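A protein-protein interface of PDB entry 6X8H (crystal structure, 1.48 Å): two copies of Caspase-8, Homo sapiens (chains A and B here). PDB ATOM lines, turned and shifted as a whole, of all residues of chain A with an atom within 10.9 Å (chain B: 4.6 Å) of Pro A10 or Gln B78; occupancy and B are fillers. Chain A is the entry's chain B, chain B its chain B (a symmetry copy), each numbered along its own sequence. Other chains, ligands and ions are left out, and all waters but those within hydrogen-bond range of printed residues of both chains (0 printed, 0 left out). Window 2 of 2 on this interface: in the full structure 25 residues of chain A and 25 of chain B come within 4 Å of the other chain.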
ATOM      1  N   ARG A   7      25.373   2.787  10.942  1.00  0.00           N
ATOM      2  CA  ARG A   7      24.905   2.443   9.608  1.00  0.00           C
ATOM      3  C   ARG A   7      25.527   3.396   8.599  1.00  0.00           C
ATOM      4  O   ARG A   7      25.856   4.540   8.939  1.00  0.00           O
ATOM      5  CB  ARG A   7      23.383   2.545   9.515  1.00  0.00           C
ATOM      6  N   TYR A   8      25.690   2.934   7.350  1.00  0.00           N
ATOM      7  CA  TYR A   8      26.234   3.800   6.291  1.00  0.00           C
ATOM      8  C   TYR A   8      25.192   4.032   5.221  1.00  0.00           C
ATOM      9  O   TYR A   8      24.436   3.125   4.887  1.00  0.00           O
ATOM     10  CB  TYR A   8      27.500   3.187   5.670  1.00  0.00           C
ATOM     11  CG  TYR A   8      28.627   3.150   6.679  1.00  0.00           C
ATOM     12  CD1 TYR A   8      28.718   2.096   7.587  1.00  0.00           C
ATOM     13  CD2 TYR A   8      29.575   4.178   6.742  1.00  0.00           C
ATOM     14  CE1 TYR A   8      29.746   2.058   8.518  1.00  0.00           C
ATOM     15  CE2 TYR A   8      30.605   4.143   7.674  1.00  0.00           C
ATOM     16  CZ  TYR A   8      30.667   3.090   8.566  1.00  0.00           C
ATOM     17  OH  TYR A   8      31.680   3.041   9.515  1.00  0.00           O
ATOM     18  N   ILE A   9      25.126   5.259   4.715  1.00  0.00           N
ATOM     19  CA  ILE A   9      24.252   5.579   3.588  1.00  0.00           C
ATOM     20  C   ILE A   9      25.123   6.248   2.531  1.00  0.00           C
ATOM     21  O   ILE A   9      26.301   6.552   2.803  1.00  0.00           O
ATOM     22  CB  ILE A   9      23.083   6.493   4.008  1.00  0.00           C
ATOM     23  CG1 ILE A   9      23.604   7.847   4.519  1.00  0.00           C
ATOM     24  CG2 ILE A   9      22.186   5.799   5.010  1.00  0.00           C
ATOM     25  CD1 ILE A   9      22.482   8.831   4.878  1.00  0.00           C
ATOM     26  N   PRO A  10      24.626   6.482   1.313  1.00  0.00           N
ATOM     27  CA  PRO A  10      25.468   7.104   0.276  1.00  0.00           C
ATOM     28  C   PRO A  10      25.837   8.544   0.590  1.00  0.00           C
ATOM     29  O   PRO A  10      25.044   9.316   1.148  1.00  0.00           O
ATOM     30  CB  PRO A  10      24.591   7.018  -0.982  1.00  0.00           C
ATOM     31  CG  PRO A  10      23.645   5.881  -0.704  1.00  0.00           C
ATOM     32  CD  PRO A  10      23.370   5.955   0.746  1.00  0.00           C
ATOM     33  N   ASP A  11      27.081   8.887   0.227  1.00  0.00           N
ATOM     34  CA  ASP A  11      27.609  10.257   0.322  1.00  0.00           C
ATOM     35  C   ASP A  11      26.638  11.298  -0.233  1.00  0.00           C
ATOM     36  O   ASP A  11      26.522  12.396   0.308  1.00  0.00           O
ATOM     37  CB  ASP A  11      28.915  10.271  -0.484  1.00  0.00           C
ATOM     38  CG  ASP A  11      29.721  11.580  -0.344  1.00  0.00           C
ATOM     39  OD1 ASP A  11      29.735  12.152   0.785  1.00  0.00           O
ATOM     40  OD2 ASP A  11      30.418  11.961  -1.331  1.00  0.00           O
ATOM     41  N   GLU A  12      25.950  10.986  -1.342  1.00  0.00           N
ATOM     42  CA  GLU A  12      25.063  11.940  -2.008  1.00  0.00           C
ATOM     43  C   GLU A  12      23.595  11.770  -1.644  1.00  0.00           C
ATOM     44  O   GLU A  12      22.726  12.277  -2.359  1.00  0.00           O
ATOM     45  CB  GLU A  12      25.279  11.957  -3.532  1.00  0.00           C
ATOM     46  CG  GLU A  12      26.729  12.278  -3.890  1.00  0.00           C
ATOM     47  CD  GLU A  12      27.034  12.304  -5.375  1.00  0.00           C
ATOM     48  OE1 GLU A  12      26.162  12.638  -6.214  1.00  0.00           O
ATOM     49  OE2 GLU A  12      28.145  11.864  -5.715  1.00  0.00           O
ATOM     50  N   ALA A  13      23.296  11.118  -0.520  1.00  0.00           N
ATOM     51  CA  ALA A  13      21.928  10.991  -0.037  1.00  0.00           C
ATOM     52  C   ALA A  13      21.356  12.318   0.467  1.00  0.00           C
ATOM     53  O   ALA A  13      22.077  13.263   0.802  1.00  0.00           O
ATOM     54  CB  ALA A  13      21.866   9.983   1.127  1.00  0.00           C
ATOM     55  N   ASP A  14      20.031  12.377   0.508  1.00  0.00           N
ATOM     56  CA  ASP A  14      19.304  13.418   1.215  1.00  0.00           C
ATOM     57  C   ASP A  14      19.410  14.768   0.553  1.00  0.00           C
ATOM     58  O   ASP A  14      19.321  15.782   1.234  1.00  0.00           O
ATOM     59  CB  ASP A  14      19.670  13.493   2.714  1.00  0.00           C
ATOM     60  CG  ASP A  14      19.684  12.109   3.377  1.00  0.00           C
ATOM     61  OD1 ASP A  14      18.634  11.436   3.300  1.00  0.00           O
ATOM     62  OD2 ASP A  14      20.737  11.725   3.963  1.00  0.00           O
ATOM     63  N   PHE A  15      19.517  14.807  -0.769  1.00  0.00           N
ATOM     64  CA  PHE A  15      19.499  16.096  -1.477  1.00  0.00           C
ATOM     65  C   PHE A  15      18.172  16.312  -2.182  1.00  0.00           C
ATOM     66  O   PHE A  15      17.519  15.377  -2.670  1.00  0.00           O
ATOM     67  CB  PHE A  15      20.589  16.153  -2.558  1.00  0.00           C
ATOM     68  CG  PHE A  15      21.961  16.522  -2.052  1.00  0.00           C
ATOM     69  CD1 PHE A  15      22.793  15.535  -1.549  1.00  0.00           C
ATOM     70  CD2 PHE A  15      22.428  17.841  -2.135  1.00  0.00           C
ATOM     71  CE1 PHE A  15      24.059  15.855  -1.086  1.00  0.00           C
ATOM     72  CE2 PHE A  15      23.689  18.179  -1.682  1.00  0.00           C
ATOM     73  CZ  PHE A  15      24.543  17.194  -1.162  1.00  0.00           C
ATOM     74  N   PHE A  84      15.880  14.479  -6.860  1.00  0.00           N
ATOM     75  CA  PHE A  84      16.066  14.241  -5.430  1.00  0.00           C
ATOM     76  C   PHE A  84      16.753  12.920  -5.109  1.00  0.00           C
ATOM     77  O   PHE A  84      16.583  11.908  -5.788  1.00  0.00           O
ATOM     78  CB  PHE A  84      14.744  14.398  -4.647  1.00  0.00           C
ATOM     79  CG  PHE A  84      13.688  13.345  -4.944  1.00  0.00           C
ATOM     80  CD1 PHE A  84      12.799  13.526  -6.015  1.00  0.00           C
ATOM     81  CD2 PHE A  84      13.515  12.236  -4.105  1.00  0.00           C
ATOM     82  CE1 PHE A  84      11.788  12.617  -6.266  1.00  0.00           C
ATOM     83  CE2 PHE A  84      12.472  11.305  -4.351  1.00  0.00           C
ATOM     84  CZ  PHE A  84      11.617  11.501  -5.444  1.00  0.00           C
ATOM     85  N   THR A  85      17.553  12.938  -4.037  1.00  0.00           N
ATOM     86  CA  THR A  85      18.018  11.713  -3.389  1.00  0.00           C
ATOM     87  C   THR A  85      17.488  11.613  -1.960  1.00  0.00           C
ATOM     88  O   THR A  85      18.053  10.893  -1.131  1.00  0.00           O
ATOM     89  CB  THR A  85      19.544  11.612  -3.438  1.00  0.00           C
ATOM     90  OG1 THR A  85      20.081  12.768  -2.792  1.00  0.00           O
ATOM     91  CG2 THR A  85      20.057  11.573  -4.886  1.00  0.00           C
ATOM     92  N   LEU A  86      16.397  12.309  -1.671  1.00  0.00           N
ATOM     93  CA  LEU A  86      15.765  12.214  -0.365  1.00  0.00           C
ATOM     94  C   LEU A  86      15.365  10.773  -0.110  1.00  0.00           C
ATOM     95  O   LEU A  86      14.894  10.078  -1.011  1.00  0.00           O
ATOM     96  CB  LEU A  86      14.499  13.078  -0.346  1.00  0.00           C
ATOM     97  CG  LEU A  86      14.675  14.574  -0.552  1.00  0.00           C
ATOM     98  CD1 LEU A  86      13.291  15.199  -0.476  1.00  0.00           C
ATOM     99  CD2 LEU A  86      15.587  15.182   0.505  1.00  0.00           C
ATOM    100  N   ARG A  87      15.556  10.339   1.136  1.00  0.00           N
ATOM    101  CA  ARG A  87      15.193   9.001   1.584  1.00  0.00           C
ATOM    102  C   ARG A  87      13.995   8.992   2.521  1.00  0.00           C
ATOM    103  O   ARG A  87      13.530   7.917   2.904  1.00  0.00           O
ATOM    104  CB  ARG A  87      16.383   8.345   2.308  1.00  0.00           C
ATOM    105  CG  ARG A  87      17.635   8.191   1.482  1.00  0.00           C
ATOM    106  CD  ARG A  87      18.824   7.761   2.394  1.00  0.00           C
ATOM    107  NE  ARG A  87      18.958   8.702   3.489  1.00  0.00           N
ATOM    108  CZ  ARG A  87      18.773   8.440   4.785  1.00  0.00           C
ATOM    109  NH1 ARG A  87      18.485   7.216   5.230  1.00  0.00           N
ATOM    110  NH2 ARG A  87      18.892   9.433   5.643  1.00  0.00           N
ATOM    111  N   ALA B  20      18.591   4.694 -11.646  1.00  0.00           N
ATOM    112  CA  ALA B  20      19.140   3.784 -10.634  1.00  0.00           C
ATOM    113  C   ALA B  20      20.287   4.395  -9.841  1.00  0.00           C
ATOM    114  O   ALA B  20      20.553   3.946  -8.718  1.00  0.00           O
ATOM    115  CB  ALA B  20      19.652   2.484 -11.278  1.00  0.00           C
ATOM    116  N   THR B  21      20.964   5.403 -10.383  1.00  0.00           N
ATOM    117  CA  THR B  21      22.104   6.002  -9.704  1.00  0.00           C
ATOM    118  C   THR B  21      22.208   7.460 -10.097  1.00  0.00           C
ATOM    119  O   THR B  21      21.838   7.840 -11.215  1.00  0.00           O
ATOM    120  CB  THR B  21      23.417   5.247 -10.033  1.00  0.00           C
ATOM    121  OG1 THR B  21      24.535   5.979  -9.494  1.00  0.00           O
ATOM    122  CG2 THR B  21      23.647   5.092 -11.561  1.00  0.00           C
ATOM    123  N   VAL B  26      28.351   3.814 -10.486  1.00  0.00           N
ATOM    124  CA  VAL B  26      27.857   2.503 -10.881  1.00  0.00           C
ATOM    125  C   VAL B  26      26.508   2.244 -10.233  1.00  0.00           C
ATOM    126  O   VAL B  26      26.129   2.859  -9.232  1.00  0.00           O
ATOM    127  CB  VAL B  26      28.857   1.391 -10.488  1.00  0.00           C
ATOM    128  CG1 VAL B  26      30.220   1.607 -11.138  1.00  0.00           C
ATOM    129  CG2 VAL B  26      28.975   1.280  -8.950  1.00  0.00           C
ATOM    130  N   SER B  27      25.756   1.301 -10.800  1.00  0.00           N
ATOM    131  CA  SER B  27      24.653   0.695 -10.089  1.00  0.00           C
ATOM    132  C   SER B  27      24.856  -0.812 -10.139  1.00  0.00           C
ATOM    133  O   SER B  27      25.561  -1.329 -11.017  1.00  0.00           O
ATOM    134  CB  SER B  27      23.313   1.068 -10.694  1.00  0.00           C
ATOM    135  OG  SER B  27      23.236   0.623 -12.032  1.00  0.00           O
ATOM    136  N   TYR B  28      24.299  -1.511  -9.173  1.00  0.00           N
ATOM    137  CA  TYR B  28      24.663  -2.890  -8.946  1.00  0.00           C
ATOM    138  C   TYR B  28      23.647  -3.875  -9.499  1.00  0.00           C
ATOM    139  O   TYR B  28      22.424  -3.660  -9.451  1.00  0.00           O
ATOM    140  CB  TYR B  28      24.830  -3.140  -7.457  1.00  0.00           C
ATOM    141  CG  TYR B  28      26.096  -2.506  -6.926  1.00  0.00           C
ATOM    142  CD1 TYR B  28      27.291  -3.208  -6.952  1.00  0.00           C
ATOM    143  CD2 TYR B  28      26.096  -1.204  -6.454  1.00  0.00           C
ATOM    144  CE1 TYR B  28      28.455  -2.636  -6.502  1.00  0.00           C
ATOM    145  CE2 TYR B  28      27.272  -0.597  -5.988  1.00  0.00           C
ATOM    146  CZ  TYR B  28      28.439  -1.342  -6.003  1.00  0.00           C
ATOM    147  OH  TYR B  28      29.607  -0.800  -5.538  1.00  0.00           O
ATOM    148  N   TRP B  36      19.849  -3.998  -7.673  1.00  0.00           N
ATOM    149  CA  TRP B  36      19.405  -3.370  -6.425  1.00  0.00           C
ATOM    150  C   TRP B  36      18.203  -2.485  -6.696  1.00  0.00           C
ATOM    151  O   TRP B  36      17.186  -2.568  -6.000  1.00  0.00           O
ATOM    152  CB  TRP B  36      20.520  -2.526  -5.795  1.00  0.00           C
ATOM    153  CG  TRP B  36      21.705  -3.298  -5.251  1.00  0.00           C
ATOM    154  CD1 TRP B  36      21.951  -4.638  -5.348  1.00  0.00           C
ATOM    155  CD2 TRP B  36      22.809  -2.732  -4.532  1.00  0.00           C
ATOM    156  NE1 TRP B  36      23.155  -4.935  -4.719  1.00  0.00           N
ATOM    157  CE2 TRP B  36      23.696  -3.779  -4.222  1.00  0.00           C
ATOM    158  CE3 TRP B  36      23.131  -1.429  -4.127  1.00  0.00           C
ATOM    159  CZ2 TRP B  36      24.895  -3.554  -3.518  1.00  0.00           C
ATOM    160  CZ3 TRP B  36      24.300  -1.214  -3.413  1.00  0.00           C
ATOM    161  CH2 TRP B  36      25.171  -2.268  -3.124  1.00  0.00           C
ATOM    162  N   TYR B  37      18.289  -1.667  -7.746  1.00  0.00           N
ATOM    163  CA  TYR B  37      17.233  -0.700  -8.007  1.00  0.00           C
ATOM    164  C   TYR B  37      15.933  -1.342  -8.506  1.00  0.00           C
ATOM    165  O   TYR B  37      14.853  -1.046  -7.979  1.00  0.00           O
ATOM    166  CB  TYR B  37      17.721   0.329  -9.007  1.00  0.00           C
ATOM    167  CG  TYR B  37      16.695   1.380  -9.362  1.00  0.00           C
ATOM    168  CD1 TYR B  37      16.279   2.295  -8.400  1.00  0.00           C
ATOM    169  CD2 TYR B  37      16.179   1.455 -10.654  1.00  0.00           C
ATOM    170  CE1 TYR B  37      15.351   3.308  -8.732  1.00  0.00           C
ATOM    171  CE2 TYR B  37      15.282   2.439 -11.016  1.00  0.00           C
ATOM    172  CZ  TYR B  37      14.873   3.360 -10.051  1.00  0.00           C
ATOM    173  OH  TYR B  37      13.987   4.382 -10.404  1.00  0.00           O
ATOM    174  N   VAL B  66      17.538   1.231  -1.082  1.00  0.00           N
ATOM    175  CA  VAL B  66      18.783   1.035  -1.819  1.00  0.00           C
ATOM    176  C   VAL B  66      19.940   1.663  -1.065  1.00  0.00           C
ATOM    177  O   VAL B  66      21.052   1.124  -1.074  1.00  0.00           O
ATOM    178  CB  VAL B  66      18.687   1.551  -3.270  1.00  0.00           C
ATOM    179  CG1 VAL B  66      20.078   1.438  -3.987  1.00  0.00           C
ATOM    180  CG2 VAL B  66      17.593   0.743  -4.038  1.00  0.00           C
ATOM    181  N   SER B  67      19.693   2.776  -0.361  1.00  0.00           N
ATOM    182  CA  SER B  67      20.740   3.416   0.425  1.00  0.00           C
ATOM    183  C   SER B  67      21.268   2.526   1.540  1.00  0.00           C
ATOM    184  O   SER B  67      22.364   2.780   2.046  1.00  0.00           O
ATOM    185  CB  SER B  67      20.232   4.714   1.057  1.00  0.00           C
ATOM    186  OG  SER B  67      20.147   5.734   0.052  1.00  0.00           O
ATOM    187  N   LYS B  77      28.425   2.021  -2.276  1.00  0.00           N
ATOM    188  CA  LYS B  77      27.005   2.279  -2.059  1.00  0.00           C
ATOM    189  C   LYS B  77      26.356   2.619  -3.392  1.00  0.00           C
ATOM    190  O   LYS B  77      27.014   2.679  -4.418  1.00  0.00           O
ATOM    191  CB  LYS B  77      26.840   3.448  -1.079  1.00  0.00           C
ATOM    192  CG  LYS B  77      27.550   3.244   0.312  1.00  0.00           C
ATOM    193  CD  LYS B  77      26.879   2.137   1.086  1.00  0.00           C
ATOM    194  CE  LYS B  77      25.609   2.627   1.750  1.00  0.00           C
ATOM    195  NZ  LYS B  77      24.921   1.506   2.516  1.00  0.00           N
ATOM    196  N   GLN B  78      25.035   2.840  -3.373  1.00  0.00           N
ATOM    197  CA  GLN B  78      24.312   3.222  -4.583  1.00  0.00           C
ATOM    198  C   GLN B  78      23.211   4.168  -4.178  1.00  0.00           C
ATOM    199  O   GLN B  78      22.453   3.881  -3.252  1.00  0.00           O
ATOM    200  CB  GLN B  78      23.659   2.002  -5.238  1.00  0.00           C
ATOM    201  CG  GLN B  78      22.960   2.333  -6.563  1.00  0.00           C
ATOM    202  CD  GLN B  78      22.438   1.111  -7.253  1.00  0.00           C
ATOM    203  OE1 GLN B  78      23.029   0.035  -7.183  1.00  0.00           O
ATOM    204  NE2 GLN B  78      21.290   1.261  -7.928  1.00  0.00           N
ATOM    205  N   MET B  79      23.122   5.293  -4.888  1.00  0.00           N
ATOM    206  CA  MET B  79      22.132   6.331  -4.581  1.00  0.00           C
ATOM    207  C   MET B  79      21.239   6.553  -5.796  1.00  0.00           C
ATOM    208  O   MET B  79      21.640   7.251  -6.744  1.00  0.00           O
ATOM    209  CB  MET B  79      22.847   7.619  -4.216  1.00  0.00           C
ATOM    210  CG  MET B  79      21.877   8.729  -3.740  1.00  0.00           C
ATOM    211  SD  MET B  79      21.097   8.305  -2.154  1.00  0.00           S
ATOM    212  CE  MET B  79      19.373   7.882  -2.587  1.00  0.00           C
ATOM    213  N   PRO B  80      20.024   6.009  -5.818  1.00  0.00           N
ATOM    214  CA  PRO B  80      19.105   6.298  -6.926  1.00  0.00           C
ATOM    215  C   PRO B  80      18.640   7.739  -6.861  1.00  0.00           C
ATOM    216  O   PRO B  80      18.841   8.462  -5.883  1.00  0.00           O
ATOM    217  CB  PRO B  80      17.937   5.325  -6.711  1.00  0.00           C
ATOM    218  CG  PRO B  80      18.498   4.236  -5.790  1.00  0.00           C
ATOM    219  CD  PRO B  80      19.477   4.998  -4.892  1.00  0.00           C
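The backbone carbonyl oxygen (O) of Glu A12 sits at hydrogen-bond distance from the side-chain hydroxyl (OG1) of Thr A85 (2.7 Å). The backbone carbonyl oxygen of Thr A85 sits at hydrogen-bond distance from the backbone NH of Asp A14, at 3.0 Å. The backbone carbonyl oxygen (O) of Phe A15 sits at hydrogen-bond distance from the backbone NH (N) of Thr A85 (2.8 Å). O of Ala B20 sits at hydrogen-bond distance from NE2 of Gln B78. The backbone NH (N) of Tyr B28 is in hydrogen-bond range of the side-chain amide oxygen (OE1) of Gln B78 (2.8 Å). The side-chain hydroxyl (OG) of Ser B67 lies close to the side-chain sulfur (SD) of Met B79 (3.5 Å).
Hydrophobic or aromatic side chains of chain A that line the printed part of chain B: Pro A10 and Ala A13. Hydrophobic or aromatic side chains of chain B within 4 Å of the printed part of chain A: Met B79. Among the printed residues, 12 pairs touch across the chains. Among the printed residues, no Asp or Glu carboxylate lies within 4 Å of a Lys or Arg side-chain nitrogen of the other chain.
No position is printed for both chains. Of the 12 pairs that touch across the chains among the printed residues, none has its exchanged pair printed and touching as well.
The backbone carbonyl oxygen (O) of Tyr A8 lies within hydrogen-bond range of the side-chain amino group (NZ) of Lys B77 (2.9 Å).
Of the printed residues of chain B, Pro A10 touches Ser B67, Gln B78 and Met B79. Of chain A, only Pro A10 comes within 4 Å of Gln B78. No residue of chain A comes within 4 Å of Ala B20. No residue of chain A comes within 4 Å of Trp B36. No residue of chain A comes within 4 Å of Val B66. Of chain A, only Pro A10, Glu A12, Ala A13 and Thr A85 come within 4 Å of Met B79. Pro B80 touches just one residue of chain A: Thr A85. Printed residues of chain B within 4 Å of Arg A87: Ser B67. Of the printed residues of chain B, Glu A12 touches Met B79. Printed residues of chain A within 4 Å of Lys B77: Tyr A8 (2.9 Å) and Ile A9 (3.7 Å). Of the printed residues of chain B, Tyr A8 touches Ser B67 and Lys B77. Of the printed residues of chain B, Thr A85 touches Met B79 (3.6 Å) and Pro B80 (3.5 Å). Leu A86 touches none of the printed residues of chain B. Phe A15 touches none of the printed residues of chain B. The nearest printed residue of chain A that does not touch Lys B77 is Pro A10 (4.002 Å).
O of Tyr A8 touches O of Ser B67 (3.5 Å). Ser B67 touches Ile A9 (O to CA, 3.7 Å). Pro A10 touches Ser B67 (CD to OG, 3.3 Å). Pro A10 touches Gln B78 (CG to O, 3.5 Å). CB of Met B79 touches CB of Pro A10, 3.7 Å away. Met B79 touches Glu A12 (CG to O, 3.9 Å). CA of Ala A13 touches SD of Met B79 (3.5 Å). Met B79 touches Thr A85. Pro B80 touches Thr A85. Arg A87 touches Ser B67.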
